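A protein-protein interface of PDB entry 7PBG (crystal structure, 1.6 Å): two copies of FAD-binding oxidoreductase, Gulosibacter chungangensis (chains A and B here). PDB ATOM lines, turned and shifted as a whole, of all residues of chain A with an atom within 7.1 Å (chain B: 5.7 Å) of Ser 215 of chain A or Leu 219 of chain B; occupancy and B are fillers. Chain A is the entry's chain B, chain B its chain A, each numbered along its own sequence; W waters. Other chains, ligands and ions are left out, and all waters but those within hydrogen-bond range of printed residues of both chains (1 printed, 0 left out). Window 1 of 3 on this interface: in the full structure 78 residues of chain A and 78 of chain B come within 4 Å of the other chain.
Ser 215 of chain A touches Gly 218 of chain B, and with the chains exchanged Gly 218 of chain A touches Ser 215 of chain B.
Ser 215 of chain A touches Leu 219 of chain B, and with the chains exchanged Leu 219 of chain A touches Ser 215 of chain B.
Ile 216 of chain A touches Leu 219 of chain B, and with the chains exchanged Leu 219 of chain A touches Ile 216 of chain B.
Leu 219 of chain A touches Ile 504 of chain B, and with the chains exchanged Ile 504 of chain A touches Leu 219 of chain B.
NE2 of Gln 211 of chain A touches OE2 of Glu 221 of chain B, at 3.9 Å.
Gly 218 of chain B touches Pro 214 of chain A.
Leu 219 of chain B touches Pro 214 of chain A (O to CB, 3.5 Å).
CG of Pro 214 of chain A touches CE2 of Phe 225 of chain B (3.9 Å).
Ser 215 of chain A touches Leu 219 of chain B.
Leu 219 of chain B touches Ile 216 of chain A.
Ser 215 of chain B touches Leu 219 of chain A.
Leu 219 of chain A touches Ile 216 of chain B (CD2 to CG2, 3.6 Å).
Leu 219 of chain A touches Ile 504 of chain B.
CD1 of Ile 504 of chain A touches CD1 of Leu 219 of chain B, at 3.9 Å.
Printed residues of chain B that touch a printed residue of chain A: Ser 215, Ile 216, Gly 218, Leu 219, Glu 221, Phe 225 and Ile 504.
Hydrophobic or aromatic side chains of chain B within 4 Å of the printed part of chain A: Ile 216, Leu 219, Phe 225 and Ile 504.
Along chain B the printed residues that touch a printed residue of chain A span positions 215 to 504.
Hydrophobic or aromatic side chains of chain A within 4 Å of the printed part of chain B: Pro 214, Ile 216, Leu 219 and Ile 504.
Along chain A the printed residues that touch a printed residue of chain B span positions 211 to 504.
Among the printed residues, no Asp or Glu carboxylate lies within 4 Å of a Lys or Arg side-chain nitrogen of the other chain.
Water W1 lies within hydrogen-bond range of the side-chain carboxylate of Glu 221 of chain B (2.6 Å) and the backbone carbonyl oxygen of Gly 213 of chain A (2.8 Å).
O of Leu 219 of chain B sits at hydrogen-bond distance from OG of Ser 223 of chain B, at 2.6 Å.
NE2 of Gln 211 of chain A is in hydrogen-bond range of O of Gly 213 of chain A (3.1 Å).
The side-chain amide nitrogen (NE2) of Gln 211 of chain A is in hydrogen-bond range of the backbone carbonyl oxygen (O) of Pro 214 of chain A (3.1 Å).
The side-chain amide nitrogen (NE2) of Gln 211 of chain A is in hydrogen-bond range of the side-chain hydroxyl (OG) of Ser 215 of chain A, at 3.1 Å.
Of the printed residues of chain B, Ile 504 of chain A touches Leu 219.
Of the printed residues of chain A, Phe 225 of chain B touches Pro 214 (3.9 Å).
The nearest residue of chain A that does not touch Leu 219 of chain B is Gly 213 of chain A (6.3 Å).
The nearest printed residue of chain B that does not touch Ile 216 of chain A is Ile 504 of chain B (4.5 Å).
O of Gly 218 of chain A lies within hydrogen-bond range of N of Ser 215 of chain B (3.0 Å).
O of Gly 218 of chain B sits at hydrogen-bond distance from N of Ser 215 of chain A.
OE2 of Glu 221 of chain B sits at hydrogen-bond distance from OG of Ser 215 of chain A (2.7 Å).
O of Gly 213 of chain A sits close to O of Glu 221 of chain B (3.5 Å).
N of Pro 214 of chain A lies close to O of Glu 221 of chain B (3.3 Å).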
ATOM      1  N   GLY A 195     -28.404  29.586 -27.276  1.00  0.00           N
ATOM      2  CA  GLY A 195     -28.777  30.997 -27.326  1.00  0.00           C
ATOM      3  C   GLY A 195     -30.167  31.184 -27.862  1.00  0.00           C
ATOM      4  O   GLY A 195     -31.121  30.472 -27.468  1.00  0.00           O
ATOM      5  N   PRO A 209     -25.095  36.252 -28.468  1.00  0.00           N
ATOM      6  CA  PRO A 209     -24.721  35.038 -27.736  1.00  0.00           C
ATOM      7  C   PRO A 209     -25.339  35.063 -26.339  1.00  0.00           C
ATOM      8  O   PRO A 209     -24.652  35.324 -25.345  1.00  0.00           O
ATOM      9  CB  PRO A 209     -23.188  35.128 -27.661  1.00  0.00           C
ATOM     10  CG  PRO A 209     -22.940  36.604 -27.591  1.00  0.00           C
ATOM     11  CD  PRO A 209     -23.982  37.225 -28.509  1.00  0.00           C
ATOM     12  N   GLY A 210     -26.635  34.879 -26.293  1.00  0.00           N
ATOM     13  CA  GLY A 210     -27.375  34.935 -25.027  1.00  0.00           C
ATOM     14  C   GLY A 210     -28.770  34.408 -25.165  1.00  0.00           C
ATOM     15  O   GLY A 210     -29.195  33.992 -26.265  1.00  0.00           O
ATOM     16  N   GLN A 211     -29.453  34.359 -24.037  1.00  0.00           N
ATOM     17  CA  GLN A 211     -30.699  33.597 -23.778  1.00  0.00           C
ATOM     18  C   GLN A 211     -31.048  33.976 -22.353  1.00  0.00           C
ATOM     19  O   GLN A 211     -30.161  34.390 -21.637  1.00  0.00           O
ATOM     20  CB  GLN A 211     -30.517  32.074 -23.870  1.00  0.00           C
ATOM     21  CG  GLN A 211     -29.490  31.516 -22.863  1.00  0.00           C
ATOM     22  CD  GLN A 211     -28.071  31.943 -23.184  1.00  0.00           C
ATOM     23  OE1 GLN A 211     -27.574  31.585 -24.230  1.00  0.00           O
ATOM     24  NE2 GLN A 211     -27.380  32.659 -22.282  1.00  0.00           N
ATOM     25  N   LEU A 212     -32.268  33.723 -21.929  1.00  0.00           N
ATOM     26  CA  LEU A 212     -32.526  33.643 -20.506  1.00  0.00           C
ATOM     27  C   LEU A 212     -31.748  32.454 -19.950  1.00  0.00           C
ATOM     28  O   LEU A 212     -31.968  31.294 -20.391  1.00  0.00           O
ATOM     29  CB  LEU A 212     -34.014  33.488 -20.255  1.00  0.00           C
ATOM     30  CG  LEU A 212     -34.367  33.697 -18.794  1.00  0.00           C
ATOM     31  CD1 LEU A 212     -34.282  35.171 -18.411  1.00  0.00           C
ATOM     32  CD2 LEU A 212     -35.738  33.117 -18.519  1.00  0.00           C
ATOM     33  N   GLY A 213     -30.914  32.711 -18.939  1.00  0.00           N
ATOM     34  CA  GLY A 213     -30.184  31.621 -18.272  1.00  0.00           C
ATOM     35  C   GLY A 213     -28.725  31.583 -18.740  1.00  0.00           C
ATOM     36  O   GLY A 213     -28.232  32.543 -19.336  1.00  0.00           O
ATOM     37  N   PRO A 214     -28.013  30.499 -18.412  1.00  0.00           N
ATOM     38  CA  PRO A 214     -26.574  30.414 -18.644  1.00  0.00           C
ATOM     39  C   PRO A 214     -26.179  30.354 -20.118  1.00  0.00           C
ATOM     40  O   PRO A 214     -26.941  29.888 -20.958  1.00  0.00           O
ATOM     41  CB  PRO A 214     -26.144  29.138 -17.932  1.00  0.00           C
ATOM     42  CG  PRO A 214     -27.420  28.309 -17.798  1.00  0.00           C
ATOM     43  CD  PRO A 214     -28.543  29.303 -17.734  1.00  0.00           C
ATOM     44  N   SER A 215     -24.983  30.850 -20.384  1.00  0.00           N
ATOM     45  CA  SER A 215     -24.326  30.805 -21.700  1.00  0.00           C
ATOM     46  C   SER A 215     -23.535  29.498 -21.727  1.00  0.00           C
ATOM     47  O   SER A 215     -22.637  29.345 -20.904  1.00  0.00           O
ATOM     48  CB  SER A 215     -23.479  32.010 -21.961  1.00  0.00           C
ATOM     49  OG  SER A 215     -24.282  33.171 -22.135  1.00  0.00           O
ATOM     50  N   ILE A 216     -23.921  28.554 -22.585  1.00  0.00           N
ATOM     51  CA  ILE A 216     -23.352  27.190 -22.522  1.00  0.00           C
ATOM     52  C   ILE A 216     -22.527  26.848 -23.756  1.00  0.00           C
ATOM     53  O   ILE A 216     -21.996  25.746 -23.753  1.00  0.00           O
ATOM     54  CB  ILE A 216     -24.439  26.134 -22.261  1.00  0.00           C
ATOM     55  CG1 ILE A 216     -25.455  26.023 -23.398  1.00  0.00           C
ATOM     56  CG2 ILE A 216     -25.115  26.440 -20.943  1.00  0.00           C
ATOM     57  CD1 ILE A 216     -26.452  24.905 -23.150  1.00  0.00           C
ATOM     58  N   GLU A 217     -22.323  27.783 -24.693  1.00  0.00           N
ATOM     59  CA  GLU A 217     -21.515  27.450 -25.900  1.00  0.00           C
ATOM     60  C   GLU A 217     -20.101  27.076 -25.466  1.00  0.00           C
ATOM     61  O   GLU A 217     -19.474  26.219 -26.083  1.00  0.00           O
ATOM     62  CB  GLU A 217     -21.503  28.592 -26.914  1.00  0.00           C
ATOM     63  CG  GLU A 217     -22.786  28.631 -27.728  1.00  0.00           C
ATOM     64  CD  GLU A 217     -22.885  29.648 -28.829  1.00  0.00           C
ATOM     65  OE1 GLU A 217     -21.903  30.296 -29.132  1.00  0.00           O
ATOM     66  OE2 GLU A 217     -23.974  29.846 -29.330  1.00  0.00           O
ATOM     67  N   GLY A 218     -19.566  27.728 -24.430  1.00  0.00           N
ATOM     68  CA  GLY A 218     -18.213  27.406 -23.981  1.00  0.00           C
ATOM     69  C   GLY A 218     -18.091  25.997 -23.445  1.00  0.00           C
ATOM     70  O   GLY A 218     -16.966  25.464 -23.429  1.00  0.00           O
ATOM     71  N   LEU A 219     -19.199  25.377 -23.015  1.00  0.00           N
ATOM     72  CA  LEU A 219     -19.178  23.985 -22.510  1.00  0.00           C
ATOM     73  C   LEU A 219     -18.727  23.041 -23.610  1.00  0.00           C
ATOM     74  O   LEU A 219     -18.247  21.957 -23.278  1.00  0.00           O
ATOM     75  CB  LEU A 219     -20.573  23.508 -22.105  1.00  0.00           C
ATOM     76  CG  LEU A 219     -21.131  23.926 -20.769  1.00  0.00           C
ATOM     77  CD1 LEU A 219     -22.322  23.022 -20.464  1.00  0.00           C
ATOM     78  CD2 LEU A 219     -20.071  23.847 -19.684  1.00  0.00           C
ATOM     79  N   ILE A 504     -20.545  17.233 -15.053  1.00  0.00           N
ATOM     80  CA  ILE A 504     -21.272  17.721 -16.246  1.00  0.00           C
ATOM     81  C   ILE A 504     -21.260  16.570 -17.262  1.00  0.00           C
ATOM     82  O   ILE A 504     -22.317  16.264 -17.858  1.00  0.00           O
ATOM     83  CB  ILE A 504     -20.660  19.017 -16.794  1.00  0.00           C
ATOM     84  CG1 ILE A 504     -20.809  20.187 -15.810  1.00  0.00           C
ATOM     85  CG2 ILE A 504     -21.240  19.353 -18.151  1.00  0.00           C
ATOM     86  CD1 ILE A 504     -19.982  21.387 -16.184  1.00  0.00           C
ATOM     87  N   HIS B 165     -25.498  39.235 -16.907  1.00  0.00           N
ATOM     88  CA  HIS B 165     -25.183  39.667 -18.281  1.00  0.00           C
ATOM     89  C   HIS B 165     -25.630  41.108 -18.423  1.00  0.00           C
ATOM     90  O   HIS B 165     -26.184  41.505 -19.474  1.00  0.00           O
ATOM     91  CB  HIS B 165     -25.816  38.758 -19.381  1.00  0.00           C
ATOM     92  CG  HIS B 165     -25.068  38.825 -20.689  1.00  0.00           C
ATOM     93  ND1 HIS B 165     -25.293  39.819 -21.638  1.00  0.00           N
ATOM     94  CD2 HIS B 165     -24.115  38.028 -21.222  1.00  0.00           C
ATOM     95  CE1 HIS B 165     -24.516  39.608 -22.690  1.00  0.00           C
ATOM     96  NE2 HIS B 165     -23.803  38.506 -22.457  1.00  0.00           N
ATOM     97  N   SER B 215     -14.955  26.038 -21.238  1.00  0.00           N
ATOM     98  CA  SER B 215     -15.041  27.401 -20.668  1.00  0.00           C
ATOM     99  C   SER B 215     -16.371  27.495 -19.933  1.00  0.00           C
ATOM    100  O   SER B 215     -17.421  27.400 -20.618  1.00  0.00           O
ATOM    101  CB  SER B 215     -14.911  28.447 -21.749  1.00  0.00           C
ATOM    102  OG  SER B 215     -13.565  28.521 -22.210  1.00  0.00           O
ATOM    103  N   ILE B 216     -16.344  27.610 -18.597  1.00  0.00           N
ATOM    104  CA  ILE B 216     -17.597  27.439 -17.801  1.00  0.00           C
ATOM    105  C   ILE B 216     -17.984  28.725 -17.045  1.00  0.00           C
ATOM    106  O   ILE B 216     -18.975  28.687 -16.338  1.00  0.00           O
ATOM    107  CB  ILE B 216     -17.476  26.251 -16.835  1.00  0.00           C
ATOM    108  CG1 ILE B 216     -16.357  26.444 -15.810  1.00  0.00           C
ATOM    109  CG2 ILE B 216     -17.312  24.981 -17.646  1.00  0.00           C
ATOM    110  CD1 ILE B 216     -16.311  25.381 -14.734  1.00  0.00           C
ATOM    111  N   GLU B 217     -17.308  29.856 -17.230  1.00  0.00           N
ATOM    112  CA  GLU B 217     -17.779  31.077 -16.499  1.00  0.00           C
ATOM    113  C   GLU B 217     -19.201  31.453 -16.953  1.00  0.00           C
ATOM    114  O   GLU B 217     -19.957  32.007 -16.119  1.00  0.00           O
ATOM    115  CB  GLU B 217     -16.861  32.274 -16.717  1.00  0.00           C
ATOM    116  CG  GLU B 217     -15.587  32.153 -15.893  1.00  0.00           C
ATOM    117  CD  GLU B 217     -14.557  33.253 -16.035  1.00  0.00           C
ATOM    118  OE1 GLU B 217     -14.884  34.343 -16.623  1.00  0.00           O
ATOM    119  OE2 GLU B 217     -13.446  33.057 -15.480  1.00  0.00           O
ATOM    120  N   GLY B 218     -19.560  31.193 -18.220  1.00  0.00           N
ATOM    121  CA  GLY B 218     -20.899  31.478 -18.741  1.00  0.00           C
ATOM    122  C   GLY B 218     -21.961  30.648 -18.047  1.00  0.00           C
ATOM    123  O   GLY B 218     -23.148  31.082 -18.041  1.00  0.00           O
ATOM    124  N   LEU B 219     -21.601  29.502 -17.432  1.00  0.00           N
ATOM    125  CA  LEU B 219     -22.596  28.710 -16.668  1.00  0.00           C
ATOM    126  C   LEU B 219     -23.109  29.501 -15.472  1.00  0.00           C
ATOM    127  O   LEU B 219     -24.201  29.203 -15.006  1.00  0.00           O
ATOM    128  CB  LEU B 219     -21.975  27.435 -16.125  1.00  0.00           C
ATOM    129  CG  LEU B 219     -21.699  26.332 -17.116  1.00  0.00           C
ATOM    130  CD1 LEU B 219     -21.386  25.072 -16.328  1.00  0.00           C
ATOM    131  CD2 LEU B 219     -22.883  26.135 -18.018  1.00  0.00           C
ATOM    132  N   PHE B 220     -22.329  30.434 -14.946  1.00  0.00           N
ATOM    133  CA  PHE B 220     -22.714  31.164 -13.714  1.00  0.00           C
ATOM    134  C   PHE B 220     -23.493  32.437 -14.060  1.00  0.00           C
ATOM    135  O   PHE B 220     -23.729  33.266 -13.139  1.00  0.00           O
ATOM    136  CB  PHE B 220     -21.473  31.437 -12.867  1.00  0.00           C
ATOM    137  CG  PHE B 220     -20.817  30.159 -12.439  1.00  0.00           C
ATOM    138  CD1 PHE B 220     -21.447  29.288 -11.566  1.00  0.00           C
ATOM    139  CD2 PHE B 220     -19.642  29.752 -13.056  1.00  0.00           C
ATOM    140  CE1 PHE B 220     -20.862  28.074 -11.249  1.00  0.00           C
ATOM    141  CE2 PHE B 220     -19.028  28.571 -12.683  1.00  0.00           C
ATOM    142  CZ  PHE B 220     -19.655  27.710 -11.809  1.00  0.00           C
ATOM    143  N   GLU B 221     -23.877  32.657 -15.316  1.00  0.00           N
ATOM    144  CA  GLU B 221     -24.681  33.848 -15.652  1.00  0.00           C
ATOM    145  C   GLU B 221     -26.173  33.507 -15.635  1.00  0.00           C
ATOM    146  O   GLU B 221     -26.606  32.505 -16.268  1.00  0.00           O
ATOM    147  CB  GLU B 221     -24.138  34.549 -16.898  1.00  0.00           C
ATOM    148  CG  GLU B 221     -24.594  33.987 -18.184  1.00  0.00           C
ATOM    149  CD  GLU B 221     -24.264  34.947 -19.319  1.00  0.00           C
ATOM    150  OE1 GLU B 221     -23.279  35.703 -19.180  1.00  0.00           O
ATOM    151  OE2 GLU B 221     -25.046  34.993 -20.256  1.00  0.00           O
ATOM    152  N   SER B 223     -28.060  32.161 -13.457  1.00  0.00           N
ATOM    153  CA  SER B 223     -28.244  30.731 -13.121  1.00  0.00           C
ATOM    154  C   SER B 223     -28.150  30.576 -11.620  1.00  0.00           C
ATOM    155  O   SER B 223     -27.954  31.570 -10.887  1.00  0.00           O
ATOM    156  CB  SER B 223     -27.192  29.897 -13.851  1.00  0.00           C
ATOM    157  OG  SER B 223     -25.917  30.252 -13.319  1.00  0.00           O
ATOM    158  N   ASN B 224     -28.320  29.341 -11.181  1.00  0.00           N
ATOM    159  CA  ASN B 224     -28.337  28.994  -9.756  1.00  0.00           C
ATOM    160  C   ASN B 224     -27.371  27.816  -9.527  1.00  0.00           C
ATOM    161  O   ASN B 224     -27.757  26.772  -8.945  1.00  0.00           O
ATOM    162  CB  ASN B 224     -29.783  28.759  -9.370  1.00  0.00           C
ATOM    163  CG  ASN B 224     -30.491  27.786 -10.286  1.00  0.00           C
ATOM    164  OD1 ASN B 224     -29.918  27.238 -11.239  1.00  0.00           O
ATOM    165  ND2 ASN B 224     -31.789  27.616 -10.025  1.00  0.00           N
ATOM    166  N   PHE B 225     -26.106  27.969  -9.916  1.00  0.00           N
ATOM    167  CA  PHE B 225     -25.135  26.849  -9.894  1.00  0.00           C
ATOM    168  C   PHE B 225     -24.000  27.103  -8.899  1.00  0.00           C
ATOM    169  O   PHE B 225     -23.312  26.156  -8.477  1.00  0.00           O
ATOM    170  CB  PHE B 225     -24.543  26.619 -11.277  1.00  0.00           C
ATOM    171  CG  PHE B 225     -25.523  26.281 -12.365  1.00  0.00           C
ATOM    172  CD1 PHE B 225     -26.784  25.768 -12.089  1.00  0.00           C
ATOM    173  CD2 PHE B 225     -25.192  26.563 -13.675  1.00  0.00           C
ATOM    174  CE1 PHE B 225     -27.648  25.457 -13.126  1.00  0.00           C
ATOM    175  CE2 PHE B 225     -26.061  26.269 -14.706  1.00  0.00           C
ATOM    176  CZ  PHE B 225     -27.279  25.712 -14.418  1.00  0.00           C
ATOM    177  N   ILE B 504     -27.691  20.145 -15.880  1.00  0.00           N
ATOM    178  CA  ILE B 504     -26.506  20.801 -15.264  1.00  0.00           C
ATOM    179  C   ILE B 504     -26.828  21.138 -13.798  1.00  0.00           C
ATOM    180  O   ILE B 504     -25.966  20.908 -12.916  1.00  0.00           O
ATOM    181  CB  ILE B 504     -26.043  22.027 -16.070  1.00  0.00           C
ATOM    182  CG1 ILE B 504     -25.584  21.619 -17.467  1.00  0.00           C
ATOM    183  CG2 ILE B 504     -24.972  22.808 -15.313  1.00  0.00           C
ATOM    184  CD1 ILE B 504     -25.566  22.767 -18.447  1.00  0.00           C
ATOM    185  N   LEU B 508     -24.738  19.846 -10.577  1.00  0.00           N
ATOM    186  CA  LEU B 508     -23.922  20.751  -9.767  1.00  0.00           C
ATOM    187  C   LEU B 508     -24.591  21.042  -8.432  1.00  0.00           C
ATOM    188  O   LEU B 508     -23.881  21.568  -7.539  1.00  0.00           O
ATOM    189  CB  LEU B 508     -23.711  22.033 -10.568  1.00  0.00           C
ATOM    190  CG  LEU B 508     -22.844  21.911 -11.819  1.00  0.00           C
ATOM    191  CD1 LEU B 508     -22.655  23.283 -12.436  1.00  0.00           C
ATOM    192  CD2 LEU B 508     -21.500  21.292 -11.510  1.00  0.00           C
HETATM  193  O   HOH W   1     -27.504  35.262 -19.531  1.00  0.00           O
